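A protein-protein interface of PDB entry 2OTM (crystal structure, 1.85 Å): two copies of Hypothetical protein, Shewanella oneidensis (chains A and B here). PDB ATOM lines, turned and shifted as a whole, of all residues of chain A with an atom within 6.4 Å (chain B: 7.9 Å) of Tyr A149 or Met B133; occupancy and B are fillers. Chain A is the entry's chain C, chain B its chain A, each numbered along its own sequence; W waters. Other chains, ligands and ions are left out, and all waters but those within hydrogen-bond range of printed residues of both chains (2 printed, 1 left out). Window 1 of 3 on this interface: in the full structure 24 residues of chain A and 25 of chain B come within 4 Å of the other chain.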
ATOM      1  N   THR A  39      -2.375 -24.767  -9.836  1.00  0.00           N
ATOM      2  CA  THR A  39      -1.179 -25.200 -10.566  1.00  0.00           C
ATOM      3  C   THR A  39      -1.391 -25.179 -12.079  1.00  0.00           C
ATOM      4  O   THR A  39      -2.507 -25.169 -12.556  1.00  0.00           O
ATOM      5  CB  THR A  39      -0.700 -26.619 -10.121  1.00  0.00           C
ATOM      6  OG1 THR A  39      -1.506 -27.639 -10.723  1.00  0.00           O
ATOM      7  CG2 THR A  39      -0.731 -26.741  -8.608  1.00  0.00           C
ATOM      8  N   SER A  40      -0.277 -25.102 -12.804  1.00  0.00           N
ATOM      9  CA  SER A  40      -0.230 -25.435 -14.205  1.00  0.00           C
ATOM     10  C   SER A  40      -0.151 -26.955 -14.293  1.00  0.00           C
ATOM     11  O   SER A  40      -0.244 -27.656 -13.286  1.00  0.00           O
ATOM     12  CB  SER A  40       0.966 -24.749 -14.863  1.00  0.00           C
ATOM     13  OG  SER A  40       0.770 -23.344 -14.918  1.00  0.00           O
ATOM     14  N   GLY A  41      -0.015 -27.483 -15.492  1.00  0.00           N
ATOM     15  CA  GLY A  41      -0.081 -28.914 -15.679  1.00  0.00           C
ATOM     16  C   GLY A  41       1.105 -29.643 -15.089  1.00  0.00           C
ATOM     17  O   GLY A  41       2.285 -29.240 -15.255  1.00  0.00           O
ATOM     18  N   GLN A  42       0.798 -30.724 -14.375  1.00  0.00           N
ATOM     19  CA  GLN A  42       1.824 -31.503 -13.693  1.00  0.00           C
ATOM     20  C   GLN A  42       1.907 -32.894 -14.273  1.00  0.00           C
ATOM     21  O   GLN A  42       0.908 -33.521 -14.518  1.00  0.00           O
ATOM     22  CB  GLN A  42       1.567 -31.585 -12.194  1.00  0.00           C
ATOM     23  CG  GLN A  42       1.463 -30.230 -11.547  1.00  0.00           C
ATOM     24  CD  GLN A  42       2.748 -29.479 -11.552  1.00  0.00           C
ATOM     25  OE1 GLN A  42       3.765 -29.998 -11.123  1.00  0.00           O
ATOM     26  NE2 GLN A  42       2.715 -28.243 -12.027  1.00  0.00           N
ATOM     27  N   ALA A  76       2.220 -32.501  -8.396  1.00  0.00           N
ATOM     28  CA  ALA A  76       1.350 -31.347  -8.149  1.00  0.00           C
ATOM     29  C   ALA A  76       1.395 -30.911  -6.682  1.00  0.00           C
ATOM     30  O   ALA A  76       1.409 -29.711  -6.398  1.00  0.00           O
ATOM     31  CB  ALA A  76      -0.090 -31.627  -8.582  1.00  0.00           C
ATOM     32  N   ARG A  95     -10.532 -28.881  -5.921  1.00  0.00           N
ATOM     33  CA  ARG A  95     -10.733 -29.306  -7.304  1.00  0.00           C
ATOM     34  C   ARG A  95      -9.482 -30.008  -7.857  1.00  0.00           C
ATOM     35  O   ARG A  95      -8.359 -29.554  -7.634  1.00  0.00           O
ATOM     36  CB  ARG A  95     -11.067 -28.069  -8.143  1.00  0.00           C
ATOM     37  CG  ARG A  95     -11.393 -28.288  -9.592  1.00  0.00           C
ATOM     38  CD  ARG A  95     -12.771 -28.802  -9.757  1.00  0.00           C
ATOM     39  NE  ARG A  95     -13.379 -28.477 -11.051  1.00  0.00           N
ATOM     40  CZ  ARG A  95     -14.690 -28.606 -11.273  1.00  0.00           C
ATOM     41  NH1 ARG A  95     -15.503 -29.013 -10.301  1.00  0.00           N
ATOM     42  NH2 ARG A  95     -15.208 -28.326 -12.468  1.00  0.00           N
ATOM     43  N   LEU A  96      -9.718 -31.118  -8.564  1.00  0.00           N
ATOM     44  CA  LEU A  96      -8.723 -31.849  -9.345  1.00  0.00           C
ATOM     45  C   LEU A  96      -9.214 -31.817 -10.785  1.00  0.00           C
ATOM     46  O   LEU A  96     -10.365 -32.096 -11.021  1.00  0.00           O
ATOM     47  CB  LEU A  96      -8.684 -33.304  -8.851  1.00  0.00           C
ATOM     48  CG  LEU A  96      -8.040 -34.396  -9.756  1.00  0.00           C
ATOM     49  CD1 LEU A  96      -6.558 -34.191  -9.875  1.00  0.00           C
ATOM     50  CD2 LEU A  96      -8.333 -35.769  -9.244  1.00  0.00           C
ATOM     51  N   GLU A  97      -8.339 -31.493 -11.746  1.00  0.00           N
ATOM     52  CA  GLU A  97      -8.683 -31.612 -13.138  1.00  0.00           C
ATOM     53  C   GLU A  97      -7.590 -32.382 -13.810  1.00  0.00           C
ATOM     54  O   GLU A  97      -6.443 -31.985 -13.706  1.00  0.00           O
ATOM     55  CB  GLU A  97      -8.874 -30.230 -13.738  1.00  0.00           C
ATOM     56  CG  GLU A  97      -9.952 -29.459 -12.976  1.00  0.00           C
ATOM     57  CD  GLU A  97     -10.319 -28.111 -13.519  1.00  0.00           C
ATOM     58  OE1 GLU A  97      -9.617 -27.538 -14.395  1.00  0.00           O
ATOM     59  OE2 GLU A  97     -11.342 -27.587 -13.020  1.00  0.00           O
ATOM     60  N   GLY A  98      -7.957 -33.468 -14.487  1.00  0.00           N
ATOM     61  CA  GLY A  98      -6.999 -34.375 -15.091  1.00  0.00           C
ATOM     62  C   GLY A  98      -7.294 -34.698 -16.540  1.00  0.00           C
ATOM     63  O   GLY A  98      -8.454 -34.821 -16.940  1.00  0.00           O
ATOM     64  N   VAL A  99      -6.222 -34.855 -17.304  1.00  0.00           N
ATOM     65  CA  VAL A  99      -6.267 -35.170 -18.739  1.00  0.00           C
ATOM     66  C   VAL A  99      -5.466 -36.448 -18.972  1.00  0.00           C
ATOM     67  O   VAL A  99      -4.346 -36.564 -18.475  1.00  0.00           O
ATOM     68  CB  VAL A  99      -5.616 -34.084 -19.612  1.00  0.00           C
ATOM     69  CG1 VAL A  99      -5.841 -34.427 -21.108  1.00  0.00           C
ATOM     70  CG2 VAL A  99      -6.146 -32.667 -19.302  1.00  0.00           C
ATOM     71  N   TRP A 135     -10.740 -35.247 -18.713  1.00  0.00           N
ATOM     72  CA  TRP A 135     -10.747 -35.142 -20.165  1.00  0.00           C
ATOM     73  C   TRP A 135      -9.858 -36.219 -20.758  1.00  0.00           C
ATOM     74  O   TRP A 135      -8.950 -36.708 -20.110  1.00  0.00           O
ATOM     75  CB  TRP A 135     -10.165 -33.800 -20.643  1.00  0.00           C
ATOM     76  CG  TRP A 135     -10.889 -32.537 -20.208  1.00  0.00           C
ATOM     77  CD1 TRP A 135     -11.989 -31.959 -20.776  1.00  0.00           C
ATOM     78  CD2 TRP A 135     -10.494 -31.694 -19.146  1.00  0.00           C
ATOM     79  NE1 TRP A 135     -12.324 -30.806 -20.091  1.00  0.00           N
ATOM     80  CE2 TRP A 135     -11.411 -30.615 -19.095  1.00  0.00           C
ATOM     81  CE3 TRP A 135      -9.466 -31.762 -18.196  1.00  0.00           C
ATOM     82  CZ2 TRP A 135     -11.307 -29.605 -18.148  1.00  0.00           C
ATOM     83  CZ3 TRP A 135      -9.335 -30.742 -17.288  1.00  0.00           C
ATOM     84  CH2 TRP A 135     -10.261 -29.678 -17.258  1.00  0.00           C
ATOM     85  N   LEU A 147      -1.822 -35.614 -17.402  1.00  0.00           N
ATOM     86  CA  LEU A 147      -1.522 -34.304 -16.857  1.00  0.00           C
ATOM     87  C   LEU A 147      -2.551 -34.029 -15.776  1.00  0.00           C
ATOM     88  O   LEU A 147      -3.740 -34.229 -16.008  1.00  0.00           O
ATOM     89  CB  LEU A 147      -1.716 -33.254 -17.930  1.00  0.00           C
ATOM     90  CG  LEU A 147      -0.576 -32.694 -18.731  1.00  0.00           C
ATOM     91  CD1 LEU A 147      -1.171 -31.571 -19.573  1.00  0.00           C
ATOM     92  CD2 LEU A 147       0.577 -32.204 -17.825  1.00  0.00           C
ATOM     93  N   VAL A 148      -2.090 -33.508 -14.647  1.00  0.00           N
ATOM     94  CA  VAL A 148      -2.909 -33.244 -13.483  1.00  0.00           C
ATOM     95  C   VAL A 148      -2.762 -31.761 -13.088  1.00  0.00           C
ATOM     96  O   VAL A 148      -1.668 -31.212 -13.121  1.00  0.00           O
ATOM     97  CB  VAL A 148      -2.457 -34.146 -12.283  1.00  0.00           C
ATOM     98  CG1 VAL A 148      -2.943 -33.600 -10.975  1.00  0.00           C
ATOM     99  CG2 VAL A 148      -2.925 -35.600 -12.506  1.00  0.00           C
ATOM    100  N   TYR A 149      -3.882 -31.146 -12.710  1.00  0.00           N
ATOM    101  CA  TYR A 149      -3.944 -29.770 -12.225  1.00  0.00           C
ATOM    102  C   TYR A 149      -4.714 -29.786 -10.898  1.00  0.00           C
ATOM    103  O   TYR A 149      -5.763 -30.437 -10.785  1.00  0.00           O
ATOM    104  CB  TYR A 149      -4.740 -28.917 -13.223  1.00  0.00           C
ATOM    105  CG  TYR A 149      -4.199 -28.798 -14.629  1.00  0.00           C
ATOM    106  CD1 TYR A 149      -4.392 -29.801 -15.559  1.00  0.00           C
ATOM    107  CD2 TYR A 149      -3.504 -27.659 -15.025  1.00  0.00           C
ATOM    108  CE1 TYR A 149      -3.880 -29.696 -16.866  1.00  0.00           C
ATOM    109  CE2 TYR A 149      -2.981 -27.535 -16.311  1.00  0.00           C
ATOM    110  CZ  TYR A 149      -3.198 -28.544 -17.234  1.00  0.00           C
ATOM    111  OH  TYR A 149      -2.778 -28.385 -18.473  1.00  0.00           O
ATOM    112  N   LEU A 150      -4.204 -29.057  -9.905  1.00  0.00           N
ATOM    113  CA  LEU A 150      -4.848 -28.947  -8.593  1.00  0.00           C
ATOM    114  C   LEU A 150      -5.199 -27.496  -8.274  1.00  0.00           C
ATOM    115  O   LEU A 150      -4.526 -26.561  -8.739  1.00  0.00           O
ATOM    116  CB  LEU A 150      -3.946 -29.507  -7.465  1.00  0.00           C
ATOM    117  CG  LEU A 150      -3.486 -30.960  -7.519  1.00  0.00           C
ATOM    118  CD1 LEU A 150      -2.704 -31.332  -6.258  1.00  0.00           C
ATOM    119  CD2 LEU A 150      -4.682 -31.875  -7.730  1.00  0.00           C
ATOM    120  N   PHE A 151      -6.296 -27.326  -7.529  1.00  0.00           N
ATOM    121  CA  PHE A 151      -6.778 -26.039  -7.062  1.00  0.00           C
ATOM    122  C   PHE A 151      -6.974 -26.147  -5.558  1.00  0.00           C
ATOM    123  O   PHE A 151      -7.652 -27.050  -5.070  1.00  0.00           O
ATOM    124  CB  PHE A 151      -8.107 -25.660  -7.704  1.00  0.00           C
ATOM    125  CG  PHE A 151      -8.077 -25.618  -9.196  1.00  0.00           C
ATOM    126  CD1 PHE A 151      -8.025 -26.797  -9.949  1.00  0.00           C
ATOM    127  CD2 PHE A 151      -8.169 -24.414  -9.858  1.00  0.00           C
ATOM    128  CE1 PHE A 151      -7.992 -26.760 -11.326  1.00  0.00           C
ATOM    129  CE2 PHE A 151      -8.160 -24.374 -11.266  1.00  0.00           C
ATOM    130  CZ  PHE A 151      -8.063 -25.551 -11.987  1.00  0.00           C
ATOM    131  N   ARG B  95      -4.523 -16.572 -15.273  1.00  0.00           N
ATOM    132  CA  ARG B  95      -4.660 -17.862 -15.915  1.00  0.00           C
ATOM    133  C   ARG B  95      -4.987 -17.732 -17.396  1.00  0.00           C
ATOM    134  O   ARG B  95      -5.789 -16.873 -17.809  1.00  0.00           O
ATOM    135  CB  ARG B  95      -5.750 -18.628 -15.212  1.00  0.00           C
ATOM    136  CG  ARG B  95      -5.978 -19.994 -15.748  1.00  0.00           C
ATOM    137  CD  ARG B  95      -5.045 -20.951 -15.142  1.00  0.00           C
ATOM    138  NE  ARG B  95      -5.664 -22.271 -15.010  1.00  0.00           N
ATOM    139  CZ  ARG B  95      -5.142 -23.255 -14.298  1.00  0.00           C
ATOM    140  NH1 ARG B  95      -3.996 -23.076 -13.659  1.00  0.00           N
ATOM    141  NH2 ARG B  95      -5.762 -24.420 -14.225  1.00  0.00           N
ATOM    142  N   LEU B  96      -4.315 -18.568 -18.185  1.00  0.00           N
ATOM    143  CA  LEU B  96      -4.575 -18.729 -19.625  1.00  0.00           C
ATOM    144  C   LEU B  96      -4.968 -20.180 -19.824  1.00  0.00           C
ATOM    145  O   LEU B  96      -4.312 -21.056 -19.289  1.00  0.00           O
ATOM    146  CB  LEU B  96      -3.315 -18.420 -20.426  1.00  0.00           C
ATOM    147  CG  LEU B  96      -3.210 -18.980 -21.844  1.00  0.00           C
ATOM    148  CD1 LEU B  96      -4.277 -18.343 -22.750  1.00  0.00           C
ATOM    149  CD2 LEU B  96      -1.829 -18.773 -22.396  1.00  0.00           C
ATOM    150  N   GLU B  97      -6.035 -20.441 -20.578  1.00  0.00           N
ATOM    151  CA  GLU B  97      -6.401 -21.814 -20.913  1.00  0.00           C
ATOM    152  C   GLU B  97      -6.619 -21.842 -22.422  1.00  0.00           C
ATOM    153  O   GLU B  97      -7.426 -21.099 -22.932  1.00  0.00           O
ATOM    154  CB  GLU B  97      -7.603 -22.316 -20.080  1.00  0.00           C
ATOM    155  CG  GLU B  97      -7.329 -22.205 -18.560  1.00  0.00           C
ATOM    156  CD  GLU B  97      -8.427 -22.749 -17.634  1.00  0.00           C
ATOM    157  OE1 GLU B  97      -9.539 -23.046 -18.096  1.00  0.00           O
ATOM    158  OE2 GLU B  97      -8.166 -22.871 -16.411  1.00  0.00           O
ATOM    159  N   GLY B  98      -5.868 -22.710 -23.096  1.00  0.00           N
ATOM    160  CA  GLY B  98      -5.860 -22.783 -24.575  1.00  0.00           C
ATOM    161  C   GLY B  98      -6.080 -24.167 -25.110  1.00  0.00           C
ATOM    162  O   GLY B  98      -5.572 -25.142 -24.548  1.00  0.00           O
ATOM    163  N   VAL B  99      -6.856 -24.243 -26.200  1.00  0.00           N
ATOM    164  CA  VAL B  99      -7.176 -25.485 -26.878  1.00  0.00           C
ATOM    165  C   VAL B  99      -6.640 -25.372 -28.307  1.00  0.00           C
ATOM    166  O   VAL B  99      -6.856 -24.357 -28.972  1.00  0.00           O
ATOM    167  CB  VAL B  99      -8.692 -25.746 -26.959  1.00  0.00           C
ATOM    168  CG1 VAL B  99      -8.961 -27.185 -27.485  1.00  0.00           C
ATOM    169  CG2 VAL B  99      -9.419 -25.463 -25.655  1.00  0.00           C
ATOM    170  N   LEU B 100      -5.944 -26.404 -28.760  1.00  0.00           N
ATOM    171  CA  LEU B 100      -5.478 -26.511 -30.129  1.00  0.00           C
ATOM    172  C   LEU B 100      -5.942 -27.804 -30.765  1.00  0.00           C
ATOM    173  O   LEU B 100      -6.092 -28.806 -30.065  1.00  0.00           O
ATOM    174  CB  LEU B 100      -3.958 -26.485 -30.147  1.00  0.00           C
ATOM    175  CG  LEU B 100      -3.305 -25.116 -29.868  1.00  0.00           C
ATOM    176  CD1 LEU B 100      -2.290 -25.192 -28.761  1.00  0.00           C
ATOM    177  CD2 LEU B 100      -2.665 -24.531 -31.154  1.00  0.00           C
ATOM    178  N   LEU B 113       1.190 -22.500 -28.054  1.00  0.00           N
ATOM    179  CA  LEU B 113       0.477 -21.738 -27.024  1.00  0.00           C
ATOM    180  C   LEU B 113       1.315 -20.637 -26.393  1.00  0.00           C
ATOM    181  O   LEU B 113       0.762 -19.691 -25.834  1.00  0.00           O
ATOM    182  CB  LEU B 113      -0.100 -22.650 -25.969  1.00  0.00           C
ATOM    183  CG  LEU B 113      -1.096 -21.991 -25.023  1.00  0.00           C
ATOM    184  CD1 LEU B 113      -2.265 -21.390 -25.743  1.00  0.00           C
ATOM    185  CD2 LEU B 113      -1.568 -23.020 -23.978  1.00  0.00           C
ATOM    186  N   SER B 117       0.972 -16.981 -24.248  1.00  0.00           N
ATOM    187  CA  SER B 117       1.726 -16.632 -23.028  1.00  0.00           C
ATOM    188  C   SER B 117       2.666 -15.445 -23.250  1.00  0.00           C
ATOM    189  O   SER B 117       2.709 -14.515 -22.424  1.00  0.00           O
ATOM    190  CB  SER B 117       2.497 -17.844 -22.481  1.00  0.00           C
ATOM    191  OG  SER B 117       1.637 -18.875 -22.004  1.00  0.00           O
ATOM    192  N   HIS B 130       1.145 -15.691 -15.517  1.00  0.00           N
ATOM    193  CA  HIS B 130      -0.036 -16.529 -15.413  1.00  0.00           C
ATOM    194  C   HIS B 130       0.336 -17.997 -15.323  1.00  0.00           C
ATOM    195  O   HIS B 130       1.382 -18.397 -15.827  1.00  0.00           O
ATOM    196  CB  HIS B 130      -0.902 -16.340 -16.675  1.00  0.00           C
ATOM    197  CG  HIS B 130      -0.174 -16.623 -17.950  1.00  0.00           C
ATOM    198  ND1 HIS B 130       0.648 -15.691 -18.556  1.00  0.00           N
ATOM    199  CD2 HIS B 130      -0.119 -17.733 -18.723  1.00  0.00           C
ATOM    200  CE1 HIS B 130       1.197 -16.235 -19.627  1.00  0.00           C
ATOM    201  NE2 HIS B 130       0.751 -17.476 -19.748  1.00  0.00           N
ATOM    202  N   SER B 131      -0.532 -18.797 -14.687  1.00  0.00           N
ATOM    203  CA  SER B 131      -0.486 -20.242 -14.848  1.00  0.00           C
ATOM    204  C   SER B 131      -1.259 -20.562 -16.115  1.00  0.00           C
ATOM    205  O   SER B 131      -1.946 -19.689 -16.675  1.00  0.00           O
ATOM    206  CB  SER B 131      -1.077 -20.959 -13.638  1.00  0.00           C
ATOM    207  OG  SER B 131      -2.387 -20.543 -13.411  1.00  0.00           O
ATOM    208  N   ARG B 132      -1.150 -21.794 -16.596  1.00  0.00           N
ATOM    209  CA  ARG B 132      -1.906 -22.148 -17.762  1.00  0.00           C
ATOM    210  C   ARG B 132      -2.293 -23.605 -17.858  1.00  0.00           C
ATOM    211  O   ARG B 132      -1.665 -24.470 -17.255  1.00  0.00           O
ATOM    212  CB  ARG B 132      -1.191 -21.669 -19.036  1.00  0.00           C
ATOM    213  CG  ARG B 132      -0.219 -22.611 -19.648  1.00  0.00           C
ATOM    214  CD  ARG B 132       0.441 -22.003 -20.900  1.00  0.00           C
ATOM    215  NE  ARG B 132       1.235 -23.022 -21.560  1.00  0.00           N
ATOM    216  CZ  ARG B 132       2.079 -22.800 -22.559  1.00  0.00           C
ATOM    217  NH1 ARG B 132       2.277 -21.582 -23.009  1.00  0.00           N
ATOM    218  NH2 ARG B 132       2.754 -23.806 -23.076  1.00  0.00           N
ATOM    219  N   MET B 133      -3.332 -23.849 -18.657  1.00  0.00           N
ATOM    220  CA  MET B 133      -3.775 -25.205 -19.027  1.00  0.00           C
ATOM    221  C   MET B 133      -3.741 -25.298 -20.542  1.00  0.00           C
ATOM    222  O   MET B 133      -3.949 -24.323 -21.216  1.00  0.00           O
ATOM    223  CB  MET B 133      -5.223 -25.491 -18.535  1.00  0.00           C
ATOM    224  CG  MET B 133      -5.502 -25.191 -17.122  1.00  0.00           C
ATOM    225  SD  MET B 133      -7.331 -25.873 -16.603  1.00  0.00           S
ATOM    226  CE  MET B 133      -7.094 -27.829 -16.539  1.00  0.00           C
ATOM    227  N   ILE B 134      -3.404 -26.469 -21.067  1.00  0.00           N
ATOM    228  CA  ILE B 134      -3.368 -26.681 -22.491  1.00  0.00           C
ATOM    229  C   ILE B 134      -4.133 -27.955 -22.796  1.00  0.00           C
ATOM    230  O   ILE B 134      -4.053 -28.895 -22.026  1.00  0.00           O
ATOM    231  CB  ILE B 134      -1.924 -26.806 -22.982  1.00  0.00           C
ATOM    232  CG1 ILE B 134      -1.842 -26.709 -24.498  1.00  0.00           C
ATOM    233  CG2 ILE B 134      -1.250 -28.098 -22.422  1.00  0.00           C
ATOM    234  CD1 ILE B 134      -0.415 -26.457 -24.997  1.00  0.00           C
ATOM    235  N   TRP B 135      -4.902 -27.951 -23.873  1.00  0.00           N
ATOM    236  CA  TRP B 135      -5.574 -29.165 -24.352  1.00  0.00           C
ATOM    237  C   TRP B 135      -5.445 -29.282 -25.838  1.00  0.00           C
ATOM    238  O   TRP B 135      -5.302 -28.277 -26.530  1.00  0.00           O
ATOM    239  CB  TRP B 135      -7.071 -29.199 -24.067  1.00  0.00           C
ATOM    240  CG  TRP B 135      -7.507 -29.099 -22.616  1.00  0.00           C
ATOM    241  CD1 TRP B 135      -7.705 -30.119 -21.718  1.00  0.00           C
ATOM    242  CD2 TRP B 135      -7.869 -27.904 -21.951  1.00  0.00           C
ATOM    243  NE1 TRP B 135      -8.147 -29.612 -20.501  1.00  0.00           N
ATOM    244  CE2 TRP B 135      -8.308 -28.254 -20.647  1.00  0.00           C
ATOM    245  CE3 TRP B 135      -7.923 -26.568 -22.348  1.00  0.00           C
ATOM    246  CZ2 TRP B 135      -8.747 -27.302 -19.736  1.00  0.00           C
ATOM    247  CZ3 TRP B 135      -8.378 -25.635 -21.445  1.00  0.00           C
ATOM    248  CH2 TRP B 135      -8.787 -26.008 -20.162  1.00  0.00           C
ATOM    249  N   LEU B 147      -8.343 -21.938 -29.678  1.00  0.00           N
ATOM    250  CA  LEU B 147      -9.295 -21.187 -28.852  1.00  0.00           C
ATOM    251  C   LEU B 147      -8.550 -20.831 -27.567  1.00  0.00           C
ATOM    252  O   LEU B 147      -7.870 -21.673 -27.016  1.00  0.00           O
ATOM    253  CB  LEU B 147     -10.454 -22.086 -28.470  1.00  0.00           C
ATOM    254  CG  LEU B 147     -11.797 -22.078 -29.151  1.00  0.00           C
ATOM    255  CD1 LEU B 147     -12.738 -23.009 -28.312  1.00  0.00           C
ATOM    256  CD2 LEU B 147     -12.322 -20.663 -29.286  1.00  0.00           C
ATOM    257  N   TYR B 149      -8.816 -18.757 -23.681  1.00  0.00           N
ATOM    258  CA  TYR B 149      -9.662 -18.280 -22.623  1.00  0.00           C
ATOM    259  C   TYR B 149      -8.743 -17.615 -21.630  1.00  0.00           C
ATOM    260  O   TYR B 149      -7.724 -18.214 -21.266  1.00  0.00           O
ATOM    261  CB  TYR B 149     -10.355 -19.464 -21.931  1.00  0.00           C
ATOM    262  CG  TYR B 149     -11.311 -20.256 -22.734  1.00  0.00           C
ATOM    263  CD1 TYR B 149     -10.869 -21.229 -23.620  1.00  0.00           C
ATOM    264  CD2 TYR B 149     -12.682 -20.099 -22.565  1.00  0.00           C
ATOM    265  CE1 TYR B 149     -11.752 -21.976 -24.347  1.00  0.00           C
ATOM    266  CE2 TYR B 149     -13.582 -20.863 -23.289  1.00  0.00           C
ATOM    267  CZ  TYR B 149     -13.101 -21.801 -24.167  1.00  0.00           C
ATOM    268  OH  TYR B 149     -13.963 -22.590 -24.811  1.00  0.00           O
ATOM    269  N   PHE B 151      -8.462 -15.379 -17.776  1.00  0.00           N
ATOM    270  CA  PHE B 151      -9.034 -15.147 -16.442  1.00  0.00           C
ATOM    271  C   PHE B 151      -8.211 -13.982 -15.834  1.00  0.00           C
ATOM    272  O   PHE B 151      -6.978 -14.033 -15.803  1.00  0.00           O
ATOM    273  CB  PHE B 151      -8.898 -16.373 -15.540  1.00  0.00           C
ATOM    274  CG  PHE B 151      -9.572 -17.591 -16.072  1.00  0.00           C
ATOM    275  CD1 PHE B 151      -8.996 -18.307 -17.125  1.00  0.00           C
ATOM    276  CD2 PHE B 151     -10.792 -18.001 -15.563  1.00  0.00           C
ATOM    277  CE1 PHE B 151      -9.626 -19.427 -17.652  1.00  0.00           C
ATOM    278  CE2 PHE B 151     -11.438 -19.130 -16.082  1.00  0.00           C
ATOM    279  CZ  PHE B 151     -10.881 -19.829 -17.120  1.00  0.00           C
HETATM  280  O   HOH W   1      -4.788 -25.791 -11.754  1.00  0.00           O
HETATM  281  O   HOH W   2      -0.114 -26.343 -18.215  1.00  0.00           O
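Among the printed residues, pairs that only touch across the chains: Ser A40 with Ser B131, Tyr A149 with Met B133, Phe A151 with Arg B95, Trp A135 with Trp B135, Tyr A149 with Arg B132, Trp A135 with Met B133, Val A99 with Trp B135 and Gly A41 with Arg B132.
Printed residues of chain B within 4 Å of Gly A41: Arg B132 (3.9 Å).
Gly A98 touches none of the printed residues of chain B.
Tyr A149 touches just these residues of chain B: Arg B132, Met B133 and Ile B134.
Of the printed residues of chain A, Arg B132 touches Ser A40, Gly A41 and Tyr A149.
Of chain A, only Glu A97 (3.3 Å), Trp A135 (3.7 Å) and Tyr A149 (3.4 Å) come within 4 Å of Met B133.
Printed residues of chain A within 4 Å of Ile B134: Tyr A149 (3.3 Å).
Leu B147 touches none of the printed residues of chain A.
The nearest residue of chain B that does not touch Tyr A149 is Arg B95 (4.03 Å).
The nearest residue of chain A that does not touch Met B133 is Phe A151 (4.7 Å).
NH1 of Arg B95 lies within hydrogen-bond range of O of Thr A39, at 2.8 Å.
OG of Ser A40 is in hydrogen-bond range of N of Arg B132.
N of Ile B134 sits at hydrogen-bond distance from OH of Tyr A149 (3.3 Å).
The side-chain carboxylate (OE1) of Glu A97 lies close to the side-chain sulfur (SD) of Met B133, 3.6 Å away.
Of the 17 printed residues of chain B, 6 touch a printed residue of chain A.
Printed residues of chain B that touch a printed residue of chain A: Arg B95, Ser B131, Arg B132, Met B133, Ile B134 and Trp B135.
Hydrophobic or aromatic side chains of chain B that line the printed part of chain A: Met B133 and Trp B135.
Of the 16 printed residues of chain A, 8 touch a printed residue of chain B.
Printed residues of chain A that touch a printed residue of chain B: Thr A39, Ser A40, Gly A41, Glu A97, Val A99, Trp A135, Tyr A149 and Phe A151.
Along chain A the printed residues that touch a printed residue of chain B span positions 39 to 151.
Water W1 lies within hydrogen-bond range of O of Thr A39, NH2 of Arg B95 and O of Leu A150.
Water W2 lies within hydrogen-bond range of O of Arg B132 (2.6 Å), N of Gly A41 (3.0 Å) and OH of Tyr A149 (3.4 Å).
The side-chain carboxylate of Glu B97 is in salt-bridge range of the guanidinium group of Arg B95 (2.9 Å).
O of Arg B95 lies within hydrogen-bond range of N of Phe B151 (3.1 Å).
The backbone NH (N) of Met B133 is in hydrogen-bond range of the backbone carbonyl oxygen (O) of Leu B96.
O of Gly B98 lies within hydrogen-bond range of N of Trp B135.
The backbone NH of Thr A39 is in hydrogen-bond range of the backbone carbonyl oxygen of Leu A150.
The backbone NH (N) of Phe A151 is in hydrogen-bond range of the backbone carbonyl oxygen (O) of Arg A95 (3.0 Å).
Val A99 touches Trp B135, but with the chains exchanged Trp A135 does not touch Val B99 (8.2 Å).
Trp A135 touches its own counterpart, Trp B135.
Phe A151 touches Arg B95, but with the chains exchanged Arg A95 does not touch Phe B151 (10.6 Å).
Positions printed for both chains: 95, 96, 97, 98, 99, 135, 147, 149 and 151.
Of the 12 pairs that touch across the chains among the printed residues, 1 has its exchanged pair printed and touching as well.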
